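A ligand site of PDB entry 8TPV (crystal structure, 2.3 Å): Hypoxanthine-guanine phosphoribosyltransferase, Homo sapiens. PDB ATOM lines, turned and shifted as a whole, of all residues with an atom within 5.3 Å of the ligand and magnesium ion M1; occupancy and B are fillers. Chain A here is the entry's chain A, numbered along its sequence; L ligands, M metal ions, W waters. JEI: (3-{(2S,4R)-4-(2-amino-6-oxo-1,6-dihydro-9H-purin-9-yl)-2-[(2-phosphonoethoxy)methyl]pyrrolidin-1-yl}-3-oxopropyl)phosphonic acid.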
ATOM      1  N   VAL A  67       5.530 -25.569 -23.232  1.00  0.00           N
ATOM      2  CA  VAL A  67       5.082 -26.678 -22.396  1.00  0.00           C
ATOM      3  C   VAL A  67       3.691 -27.128 -22.879  1.00  0.00           C
ATOM      4  O   VAL A  67       2.672 -26.485 -22.601  1.00  0.00           O
ATOM      5  CB  VAL A  67       5.063 -26.294 -20.910  1.00  0.00           C
ATOM      6  CG1 VAL A  67       4.641 -27.509 -20.078  1.00  0.00           C
ATOM      7  CG2 VAL A  67       6.465 -25.785 -20.473  1.00  0.00           C
ATOM      8  N   LEU A  68       3.659 -28.260 -23.581  1.00  0.00           N
ATOM      9  CA  LEU A  68       2.418 -28.820 -24.099  1.00  0.00           C
ATOM     10  C   LEU A  68       1.668 -29.587 -23.009  1.00  0.00           C
ATOM     11  O   LEU A  68       2.221 -29.951 -21.971  1.00  0.00           O
ATOM     12  CB  LEU A  68       2.707 -29.728 -25.296  1.00  0.00           C
ATOM     13  CG  LEU A  68       3.610 -29.200 -26.400  1.00  0.00           C
ATOM     14  CD1 LEU A  68       4.176 -30.365 -27.168  1.00  0.00           C
ATOM     15  CD2 LEU A  68       2.857 -28.268 -27.322  1.00  0.00           C
ATOM     16  N   LYS A  69       0.383 -29.827 -23.258  1.00  0.00           N
ATOM     17  CA  LYS A  69      -0.354 -29.341 -24.428  1.00  0.00           C
ATOM     18  C   LYS A  69      -0.912 -27.949 -24.199  1.00  0.00           C
ATOM     19  O   LYS A  69      -1.018 -27.155 -25.138  1.00  0.00           O
ATOM     20  CB  LYS A  69      -1.502 -30.275 -24.780  1.00  0.00           C
ATOM     21  CG  LYS A  69      -1.096 -31.710 -25.103  1.00  0.00           C
ATOM     22  CD  LYS A  69      -2.349 -32.495 -25.397  1.00  0.00           C
ATOM     23  CE  LYS A  69      -2.103 -33.987 -25.528  1.00  0.00           C
ATOM     24  NZ  LYS A  69      -3.401 -34.731 -25.557  1.00  0.00           N
ATOM     25  N   GLY A  70      -1.271 -27.654 -22.934  1.00  0.00           N
ATOM     26  CA  GLY A  70      -1.984 -26.421 -22.628  1.00  0.00           C
ATOM     27  C   GLY A  70      -1.339 -25.164 -23.186  1.00  0.00           C
ATOM     28  O   GLY A  70      -2.026 -24.183 -23.465  1.00  0.00           O
ATOM     29  N   GLY A  71      -0.022 -25.163 -23.340  1.00  0.00           N
ATOM     30  CA  GLY A  71       0.636 -23.941 -23.744  1.00  0.00           C
ATOM     31  C   GLY A  71       0.701 -23.676 -25.221  1.00  0.00           C
ATOM     32  O   GLY A  71       1.212 -22.625 -25.618  1.00  0.00           O
ATOM     33  N   ASP A 135       0.810 -22.243 -20.057  1.00  0.00           N
ATOM     34  CA  ASP A 135      -0.555 -21.730 -20.004  1.00  0.00           C
ATOM     35  C   ASP A 135      -0.913 -21.234 -18.606  1.00  0.00           C
ATOM     36  O   ASP A 135      -1.414 -20.120 -18.453  1.00  0.00           O
ATOM     37  CB  ASP A 135      -1.569 -22.790 -20.462  1.00  0.00           C
ATOM     38  CG  ASP A 135      -1.369 -24.130 -19.758  1.00  0.00           C
ATOM     39  OD1 ASP A 135      -0.287 -24.349 -19.172  1.00  0.00           O
ATOM     40  OD2 ASP A 135      -2.279 -24.980 -19.812  1.00  0.00           O
ATOM     41  N   ILE A 136      -0.680 -22.038 -17.581  1.00  0.00           N
ATOM     42  CA  ILE A 136      -1.150 -21.690 -16.247  1.00  0.00           C
ATOM     43  C   ILE A 136      -0.127 -22.115 -15.189  1.00  0.00           C
ATOM     44  O   ILE A 136       0.555 -23.133 -15.316  1.00  0.00           O
ATOM     45  CB  ILE A 136      -2.550 -22.303 -15.980  1.00  0.00           C
ATOM     46  CG1 ILE A 136      -3.130 -21.777 -14.663  1.00  0.00           C
ATOM     47  CG2 ILE A 136      -2.497 -23.798 -15.925  1.00  0.00           C
ATOM     48  CD1 ILE A 136      -4.585 -22.168 -14.421  1.00  0.00           C
ATOM     49  N   ILE A 137      -0.006 -21.296 -14.152  1.00  0.00           N
ATOM     50  CA  ILE A 137       0.754 -21.608 -12.959  1.00  0.00           C
ATOM     51  C   ILE A 137      -0.230 -21.678 -11.802  1.00  0.00           C
ATOM     52  O   ILE A 137      -0.976 -20.729 -11.559  1.00  0.00           O
ATOM     53  CB  ILE A 137       1.855 -20.569 -12.693  1.00  0.00           C
ATOM     54  CG1 ILE A 137       2.969 -20.743 -13.735  1.00  0.00           C
ATOM     55  CG2 ILE A 137       2.401 -20.732 -11.277  1.00  0.00           C
ATOM     56  CD1 ILE A 137       4.126 -19.813 -13.525  1.00  0.00           C
ATOM     57  N   ASP A 138      -0.271 -22.832 -11.113  1.00  0.00           N
ATOM     58  CA  ASP A 138      -1.197 -23.023 -10.007  1.00  0.00           C
ATOM     59  C   ASP A 138      -0.409 -23.007  -8.699  1.00  0.00           C
ATOM     60  O   ASP A 138      -0.183 -21.912  -8.130  1.00  0.00           O
ATOM     61  CB  ASP A 138      -2.000 -24.304 -10.227  1.00  0.00           C
ATOM     62  CG  ASP A 138      -3.115 -24.444  -9.237  1.00  0.00           C
ATOM     63  OD1 ASP A 138      -3.335 -23.487  -8.468  1.00  0.00           O
ATOM     64  OD2 ASP A 138      -3.761 -25.520  -9.214  1.00  0.00           O
ATOM     65  N   THR A 139       0.028 -24.164  -8.169  1.00  0.00           N
ATOM     66  CA  THR A 139       0.909 -24.168  -6.997  1.00  0.00           C
ATOM     67  C   THR A 139       2.304 -23.667  -7.328  1.00  0.00           C
ATOM     68  O   THR A 139       3.018 -23.232  -6.421  1.00  0.00           O
ATOM     69  CB  THR A 139       1.066 -25.575  -6.386  1.00  0.00           C
ATOM     70  OG1 THR A 139       1.705 -26.478  -7.308  1.00  0.00           O
ATOM     71  CG2 THR A 139      -0.265 -26.163  -5.948  1.00  0.00           C
ATOM     72  N   GLY A 140       2.728 -23.728  -8.587  1.00  0.00           N
ATOM     73  CA  GLY A 140       4.085 -23.408  -8.953  1.00  0.00           C
ATOM     74  C   GLY A 140       5.088 -24.511  -8.734  1.00  0.00           C
ATOM     75  O   GLY A 140       6.269 -24.329  -9.061  1.00  0.00           O
ATOM     76  N   LYS A 141       4.672 -25.661  -8.197  1.00  0.00           N
ATOM     77  CA  LYS A 141       5.648 -26.720  -7.937  1.00  0.00           C
ATOM     78  C   LYS A 141       6.260 -27.246  -9.224  1.00  0.00           C
ATOM     79  O   LYS A 141       7.484 -27.416  -9.318  1.00  0.00           O
ATOM     80  CB  LYS A 141       5.012 -27.856  -7.125  1.00  0.00           C
ATOM     81  CG  LYS A 141       4.927 -27.536  -5.623  1.00  0.00           C
ATOM     82  CD  LYS A 141       3.984 -28.468  -4.874  1.00  0.00           C
ATOM     83  CE  LYS A 141       2.523 -28.200  -5.217  1.00  0.00           C
ATOM     84  NZ  LYS A 141       1.769 -29.464  -5.505  1.00  0.00           N
ATOM     85  N   THR A 142       5.433 -27.474 -10.247  1.00  0.00           N
ATOM     86  CA  THR A 142       5.940 -27.976 -11.521  1.00  0.00           C
ATOM     87  C   THR A 142       6.999 -27.047 -12.108  1.00  0.00           C
ATOM     88  O   THR A 142       8.068 -27.500 -12.521  1.00  0.00           O
ATOM     89  CB  THR A 142       4.789 -28.170 -12.506  1.00  0.00           C
ATOM     90  OG1 THR A 142       3.862 -29.100 -11.944  1.00  0.00           O
ATOM     91  CG2 THR A 142       5.321 -28.715 -13.835  1.00  0.00           C
ATOM     92  N   MET A 143       6.712 -25.754 -12.130  1.00  0.00           N
ATOM     93  CA  MET A 143       7.651 -24.809 -12.716  1.00  0.00           C
ATOM     94  C   MET A 143       8.965 -24.790 -11.945  1.00  0.00           C
ATOM     95  O   MET A 143      10.040 -24.707 -12.536  1.00  0.00           O
ATOM     96  CB  MET A 143       7.017 -23.416 -12.760  1.00  0.00           C
ATOM     97  CG  MET A 143       7.531 -22.478 -13.845  1.00  0.00           C
ATOM     98  SD  MET A 143       8.202 -23.252 -15.345  1.00  0.00           S
ATOM     99  CE  MET A 143       6.755 -24.078 -16.015  1.00  0.00           C
ATOM    100  N   LYS A 166      -2.652 -18.361 -10.920  1.00  0.00           N
ATOM    101  CA  LYS A 166      -3.805 -18.545 -10.044  1.00  0.00           C
ATOM    102  C   LYS A 166      -3.477 -18.098  -8.611  1.00  0.00           C
ATOM    103  O   LYS A 166      -2.447 -18.487  -8.049  1.00  0.00           O
ATOM    104  CB  LYS A 166      -4.224 -20.010 -10.123  1.00  0.00           C
ATOM    105  CG  LYS A 166      -5.495 -20.366  -9.423  1.00  0.00           C
ATOM    106  CD  LYS A 166      -5.907 -21.786  -9.768  1.00  0.00           C
ATOM    107  CE  LYS A 166      -6.494 -21.904 -11.143  1.00  0.00           C
ATOM    108  NZ  LYS A 166      -7.254 -23.183 -11.182  1.00  0.00           N
ATOM    109  N   ARG A 170      -2.347 -22.655  -1.823  1.00  0.00           N
ATOM    110  CA  ARG A 170      -1.417 -23.746  -2.039  1.00  0.00           C
ATOM    111  C   ARG A 170      -0.162 -23.333  -2.802  1.00  0.00           C
ATOM    112  O   ARG A 170       0.648 -24.203  -3.117  1.00  0.00           O
ATOM    113  CB  ARG A 170      -2.126 -24.866  -2.797  1.00  0.00           C
ATOM    114  CG  ARG A 170      -3.484 -25.184  -2.181  1.00  0.00           C
ATOM    115  CD  ARG A 170      -4.071 -26.463  -2.745  1.00  0.00           C
ATOM    116  NE  ARG A 170      -4.071 -26.415  -4.204  1.00  0.00           N
ATOM    117  CZ  ARG A 170      -3.640 -27.374  -5.010  1.00  0.00           C
ATOM    118  NH1 ARG A 170      -3.219 -28.547  -4.551  1.00  0.00           N
ATOM    119  NH2 ARG A 170      -3.655 -27.163  -6.328  1.00  0.00           N
ATOM    120  N   LYS A 186     -10.115 -20.701  -9.382  1.00  0.00           N
ATOM    121  CA  LYS A 186     -11.230 -21.282 -10.123  1.00  0.00           C
ATOM    122  C   LYS A 186     -10.691 -22.186 -11.241  1.00  0.00           C
ATOM    123  O   LYS A 186      -9.602 -21.946 -11.773  1.00  0.00           O
ATOM    124  CB  LYS A 186     -12.131 -20.191 -10.741  1.00  0.00           C
ATOM    125  CG  LYS A 186     -13.150 -19.570  -9.784  1.00  0.00           C
ATOM    126  CD  LYS A 186     -14.326 -18.922 -10.552  1.00  0.00           C
ATOM    127  CE  LYS A 186     -15.688 -19.488 -10.090  1.00  0.00           C
ATOM    128  NZ  LYS A 186     -16.769 -19.482 -11.155  1.00  0.00           N
ATOM    129  N   PHE A 187     -11.439 -23.224 -11.599  1.00  0.00           N
ATOM    130  CA  PHE A 187     -11.039 -24.063 -12.719  1.00  0.00           C
ATOM    131  C   PHE A 187     -11.566 -23.430 -14.009  1.00  0.00           C
ATOM    132  O   PHE A 187     -12.771 -23.225 -14.157  1.00  0.00           O
ATOM    133  CB  PHE A 187     -11.539 -25.497 -12.584  1.00  0.00           C
ATOM    134  CG  PHE A 187     -10.806 -26.475 -13.494  1.00  0.00           C
ATOM    135  CD1 PHE A 187      -9.547 -26.950 -13.157  1.00  0.00           C
ATOM    136  CD2 PHE A 187     -11.383 -26.890 -14.695  1.00  0.00           C
ATOM    137  CE1 PHE A 187      -8.857 -27.849 -14.011  1.00  0.00           C
ATOM    138  CE2 PHE A 187     -10.711 -27.776 -15.549  1.00  0.00           C
ATOM    139  CZ  PHE A 187      -9.439 -28.256 -15.209  1.00  0.00           C
ATOM    140  N   VAL A 188     -10.654 -23.102 -14.927  1.00  0.00           N
ATOM    141  CA  VAL A 188     -10.998 -22.482 -16.197  1.00  0.00           C
ATOM    142  C   VAL A 188     -10.614 -23.443 -17.329  1.00  0.00           C
ATOM    143  O   VAL A 188      -9.710 -24.278 -17.193  1.00  0.00           O
ATOM    144  CB  VAL A 188     -10.296 -21.125 -16.398  1.00  0.00           C
ATOM    145  CG1 VAL A 188     -10.855 -20.074 -15.440  1.00  0.00           C
ATOM    146  CG2 VAL A 188      -8.825 -21.277 -16.168  1.00  0.00           C
ATOM    147  N   VAL A 189     -11.300 -23.288 -18.456  1.00  0.00           N
ATOM    148  CA  VAL A 189     -10.997 -24.041 -19.675  1.00  0.00           C
ATOM    149  C   VAL A 189     -10.878 -23.081 -20.846  1.00  0.00           C
ATOM    150  O   VAL A 189     -11.279 -21.925 -20.770  1.00  0.00           O
ATOM    151  CB  VAL A 189     -12.045 -25.113 -20.001  1.00  0.00           C
ATOM    152  CG1 VAL A 189     -12.017 -26.196 -18.954  1.00  0.00           C
ATOM    153  CG2 VAL A 189     -13.427 -24.462 -20.206  1.00  0.00           C
ATOM    154  N   LEU A 193      -6.476 -24.686 -22.652  1.00  0.00           N
ATOM    155  CA  LEU A 193      -6.646 -25.304 -21.346  1.00  0.00           C
ATOM    156  C   LEU A 193      -7.804 -26.277 -21.415  1.00  0.00           C
ATOM    157  O   LEU A 193      -8.855 -25.972 -22.005  1.00  0.00           O
ATOM    158  CB  LEU A 193      -6.911 -24.253 -20.276  1.00  0.00           C
ATOM    159  CG  LEU A 193      -5.755 -23.426 -19.757  1.00  0.00           C
ATOM    160  CD1 LEU A 193      -5.302 -22.462 -20.817  1.00  0.00           C
ATOM    161  CD2 LEU A 193      -6.269 -22.637 -18.571  1.00  0.00           C
ATOM    162  N   ASP A 194      -7.652 -27.439 -20.788  1.00  0.00           N
ATOM    163  CA  ASP A 194      -8.592 -28.540 -21.011  1.00  0.00           C
ATOM    164  C   ASP A 194      -9.247 -29.006 -19.725  1.00  0.00           C
ATOM    165  O   ASP A 194      -8.750 -28.786 -18.617  1.00  0.00           O
ATOM    166  CB  ASP A 194      -7.907 -29.752 -21.631  1.00  0.00           C
ATOM    167  CG  ASP A 194      -7.119 -30.530 -20.589  1.00  0.00           C
ATOM    168  OD1 ASP A 194      -6.230 -29.898 -19.971  1.00  0.00           O
ATOM    169  OD2 ASP A 194      -7.371 -31.746 -20.376  1.00  0.00           O
ATOM    170  N   TYR A 195     -10.345 -29.726 -19.909  1.00  0.00           N
ATOM    171  CA  TYR A 195     -10.961 -30.542 -18.887  1.00  0.00           C
ATOM    172  C   TYR A 195     -11.044 -31.947 -19.470  1.00  0.00           C
ATOM    173  O   TYR A 195     -11.920 -32.235 -20.284  1.00  0.00           O
ATOM    174  CB  TYR A 195     -12.337 -30.014 -18.530  1.00  0.00           C
ATOM    175  CG  TYR A 195     -13.039 -30.844 -17.497  1.00  0.00           C
ATOM    176  CD1 TYR A 195     -12.524 -30.955 -16.206  1.00  0.00           C
ATOM    177  CD2 TYR A 195     -14.208 -31.505 -17.795  1.00  0.00           C
ATOM    178  CE1 TYR A 195     -13.172 -31.703 -15.234  1.00  0.00           C
ATOM    179  CE2 TYR A 195     -14.865 -32.268 -16.838  1.00  0.00           C
ATOM    180  CZ  TYR A 195     -14.354 -32.364 -15.566  1.00  0.00           C
ATOM    181  OH  TYR A 195     -15.029 -33.133 -14.634  1.00  0.00           O
ATOM    182  N   GLU A 197      -9.041 -33.300 -21.696  1.00  0.00           N
ATOM    183  CA  GLU A 197      -8.750 -33.217 -23.125  1.00  0.00           C
ATOM    184  C   GLU A 197      -9.768 -32.361 -23.868  1.00  0.00           C
ATOM    185  O   GLU A 197      -9.467 -31.839 -24.960  1.00  0.00           O
ATOM    186  CB  GLU A 197      -8.665 -34.616 -23.748  1.00  0.00           C
ATOM    187  CG  GLU A 197      -7.468 -35.395 -23.214  1.00  0.00           C
ATOM    188  CD  GLU A 197      -6.192 -34.520 -23.084  1.00  0.00           C
ATOM    189  OE1 GLU A 197      -5.943 -33.665 -23.969  1.00  0.00           O
ATOM    190  OE2 GLU A 197      -5.443 -34.679 -22.096  1.00  0.00           O
ATOM    191  N   ARG A 200     -10.109 -27.647 -25.386  1.00  0.00           N
ATOM    192  CA  ARG A 200      -8.943 -26.974 -25.957  1.00  0.00           C
ATOM    193  C   ARG A 200      -9.340 -26.198 -27.202  1.00  0.00           C
ATOM    194  O   ARG A 200      -8.781 -25.125 -27.469  1.00  0.00           O
ATOM    195  CB  ARG A 200      -7.819 -27.967 -26.296  1.00  0.00           C
ATOM    196  CG  ARG A 200      -7.212 -28.625 -25.072  1.00  0.00           C
ATOM    197  CD  ARG A 200      -5.780 -29.148 -25.266  1.00  0.00           C
ATOM    198  NE  ARG A 200      -5.509 -30.271 -24.355  1.00  0.00           N
ATOM    199  CZ  ARG A 200      -4.964 -30.145 -23.152  1.00  0.00           C
ATOM    200  NH1 ARG A 200      -4.614 -28.978 -22.654  1.00  0.00           N
ATOM    201  NH2 ARG A 200      -4.775 -31.239 -22.408  1.00  0.00           N
HETATM  202  C10 JEI L   1      -3.613 -27.895 -13.902  1.00  0.00           C
HETATM  203  C15 JEI L   1      -6.266 -25.406 -13.689  1.00  0.00           C
HETATM  204  C22 JEI L   1      -2.577 -27.253 -14.299  1.00  0.00           C
HETATM  205  C24 JEI L   1      -0.508 -28.651 -14.914  1.00  0.00           C
HETATM  206  C26 JEI L   1       0.908 -27.566 -13.304  1.00  0.00           C
HETATM  207  C05 JEI L   1      -1.285 -31.252 -18.676  1.00  0.00           C
HETATM  208  C06 JEI L   1      -1.083 -30.309 -17.475  1.00  0.00           C
HETATM  209  C07 JEI L   1      -2.433 -30.194 -16.764  1.00  0.00           C
HETATM  210  C09 JEI L   1      -3.990 -28.909 -15.071  1.00  0.00           C
HETATM  211  C12 JEI L   1      -4.675 -26.104 -12.427  1.00  0.00           C
HETATM  212  C14 JEI L   1      -5.593 -26.379 -14.378  1.00  0.00           C
HETATM  213  C16 JEI L   1      -7.430 -24.724 -14.374  1.00  0.00           C
HETATM  214  C18 JEI L   1      -7.088 -26.152 -16.387  1.00  0.00           C
HETATM  215  C23 JEI L   1      -1.841 -28.166 -15.465  1.00  0.00           C
HETATM  216  C27 JEI L   1       0.444 -26.505 -12.318  1.00  0.00           C
HETATM  217  N08 JEI L   1      -2.676 -29.145 -15.802  1.00  0.00           N
HETATM  218  N11 JEI L   1      -4.631 -26.810 -13.578  1.00  0.00           N
HETATM  219  N13 JEI L   1      -5.683 -25.250 -12.499  1.00  0.00           N
HETATM  220  N17 JEI L   1      -7.809 -25.114 -15.693  1.00  0.00           N
HETATM  221  N19 JEI L   1      -7.440 -26.582 -17.717  1.00  0.00           N
HETATM  222  N20 JEI L   1      -5.979 -26.784 -15.749  1.00  0.00           N
HETATM  223  O01 JEI L   1      -1.157 -29.130 -20.469  1.00  0.00           O
HETATM  224  O03 JEI L   1      -3.410 -30.061 -19.992  1.00  0.00           O
HETATM  225  O04 JEI L   1      -1.795 -31.328 -21.382  1.00  0.00           O
HETATM  226  O21 JEI L   1      -8.011 -23.869 -13.794  1.00  0.00           O
HETATM  227  O25 JEI L   1      -0.283 -28.288 -13.576  1.00  0.00           O
HETATM  228  O29 JEI L   1       2.430 -27.439 -10.498  1.00  0.00           O
HETATM  229  O30 JEI L   1       1.897 -24.981 -10.737  1.00  0.00           O
HETATM  230  O31 JEI L   1       0.338 -26.557  -9.597  1.00  0.00           O
HETATM  231  O32 JEI L   1      -3.298 -30.979 -16.975  1.00  0.00           O
HETATM  232  P02 JEI L   1      -1.939 -30.390 -20.194  1.00  0.00           P
HETATM  233  P28 JEI L   1       1.355 -26.391 -10.699  1.00  0.00           P
HETATM  234 MG    MG M   1      -4.876 -30.367 -18.170  1.00  0.00          MG
HETATM  235 MG    MG M   2       0.868 -26.174 -18.492  1.00  0.00          MG
HETATM  236  O   HOH W   1      -6.653 -30.367 -17.247  1.00  0.00           O
HETATM  237  O   HOH W   2      -5.145 -32.285 -18.837  1.00  0.00           O
HETATM  238  O   HOH W   3      -0.830 -26.914 -18.476  1.00  0.00           O
HETATM  239  O   HOH W   4      -2.945 -33.846 -21.165  1.00  0.00           O
HETATM  240  O   HOH W   5       1.029 -26.909 -20.766  1.00  0.00           O
HETATM  241  O   HOH W   6      -4.789 -28.107 -18.076  1.00  0.00           O
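The backbone NH of Gly 70 sits at hydrogen-bond distance from an oxygen (O01) of the ligand (2.9 Å). The backbone NH of Asp 138 lies within hydrogen-bond range of an oxygen (O30) of the ligand (3.1 Å). O of Val 188 sits at hydrogen-bond distance from N17 of the ligand (2.6 Å). An oxygen (O31) of the ligand is in hydrogen-bond range of the side-chain hydroxyl (OG1) of Thr 139 (2.7 Å). The backbone NH of Gly 140 lies within hydrogen-bond range of an oxygen (O30) of the ligand (2.6 Å). N of Val 188 sits at hydrogen-bond distance from O21 of the ligand. NZ of Lys 166 lies within hydrogen-bond range of O21 of the ligand, at 2.8 Å. An oxygen (O29) of the ligand lies within hydrogen-bond range of the side-chain hydroxyl (OG1) of Thr 142 (2.6 Å). The backbone NH (N) of Lys 69 sits at hydrogen-bond distance from an oxygen (O04) of the ligand (3.2 Å). O04 of the ligand lies within salt-bridge range of NH2 of Arg 200. N of Thr 139 is in hydrogen-bond range of O31 of the ligand, 2.8 Å away. The backbone carbonyl oxygen (O) of Asp 194 is in hydrogen-bond range of a nitrogen (N19) of the ligand (2.7 Å). N of Thr 142 sits at hydrogen-bond distance from O29 of the ligand.
The side-chain carboxylate of Asp 194 sits at hydrogen-bond distance from the backbone NH of Glu 197 (2.6 Å). The side-chain amino group (NZ) of Lys 69 is in salt-bridge range of the side-chain carboxylate (OE1) of Glu 197, 3.2 Å away. OD2 of Asp 194 is in salt-bridge range of NH2 of Arg 200, at 3.3 Å. The backbone NH (N) of Lys 166 lies within hydrogen-bond range of the backbone carbonyl oxygen (O) of Ile 137 (3.0 Å). OD2 of Asp 138 is in salt-bridge range of NH2 of Arg 170 (3.3 Å). The guanidinium group (NH2) of Arg 200 is in salt-bridge range of the side-chain carboxylate (OE1) of Glu 197, at 3.1 Å. OG1 of Thr 139 sits close to N of Lys 141 (3.2 Å). NZ of Lys 166 sits at hydrogen-bond distance from O of Lys 186, at 2.7 Å.
An oxygen (O21) of the ligand lies close to the backbone carbonyl oxygen (O) of Lys 186, 3.2 Å away. Leu 68 touches the ligand. Ile 136 touches the ligand. Lys 141 touches the ligand (N to O29, 3.7 Å). CA of Phe 187 touches O21 of the ligand, 3.2 Å away. Leu 193 touches the ligand (CB to N19, 3.5 Å).
Of the 25 residues printed, 1 comes within 4 Å of magnesium ion M1. The nearest printed residue that does not touch magnesium ion M1 is Arg 200 (4.3 Å).
Magnesium ion M1 is bound by water W1 (2.0 Å), water W2 (2.0 Å), an oxygen (O32) of the ligand (2.1 Å), water W6 (2.3 Å), the side-chain carboxylate (OD1) of Asp 194 (2.3 Å) and an oxygen (O03) of the ligand (2.4 Å). Magnesium ion M1 has six donor atoms within binding distance.
Water W4 lies within hydrogen-bond range of O04 of the ligand (2.8 Å), OE2 of Glu 197 (2.8 Å) and NH2 of Arg 200 (3.4 Å). Water W3 lies within hydrogen-bond range of OD2 of Asp 135 (2.8 Å) and O01 of the ligand (3.0 Å). Water W5 lies within hydrogen-bond range of O of Val 67 (2.5 Å), O01 of the ligand (3.1 Å), N of Gly 70 (3.2 Å), N of Gly 71 (3.3 Å) and O of Leu 68 (3.5 Å).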
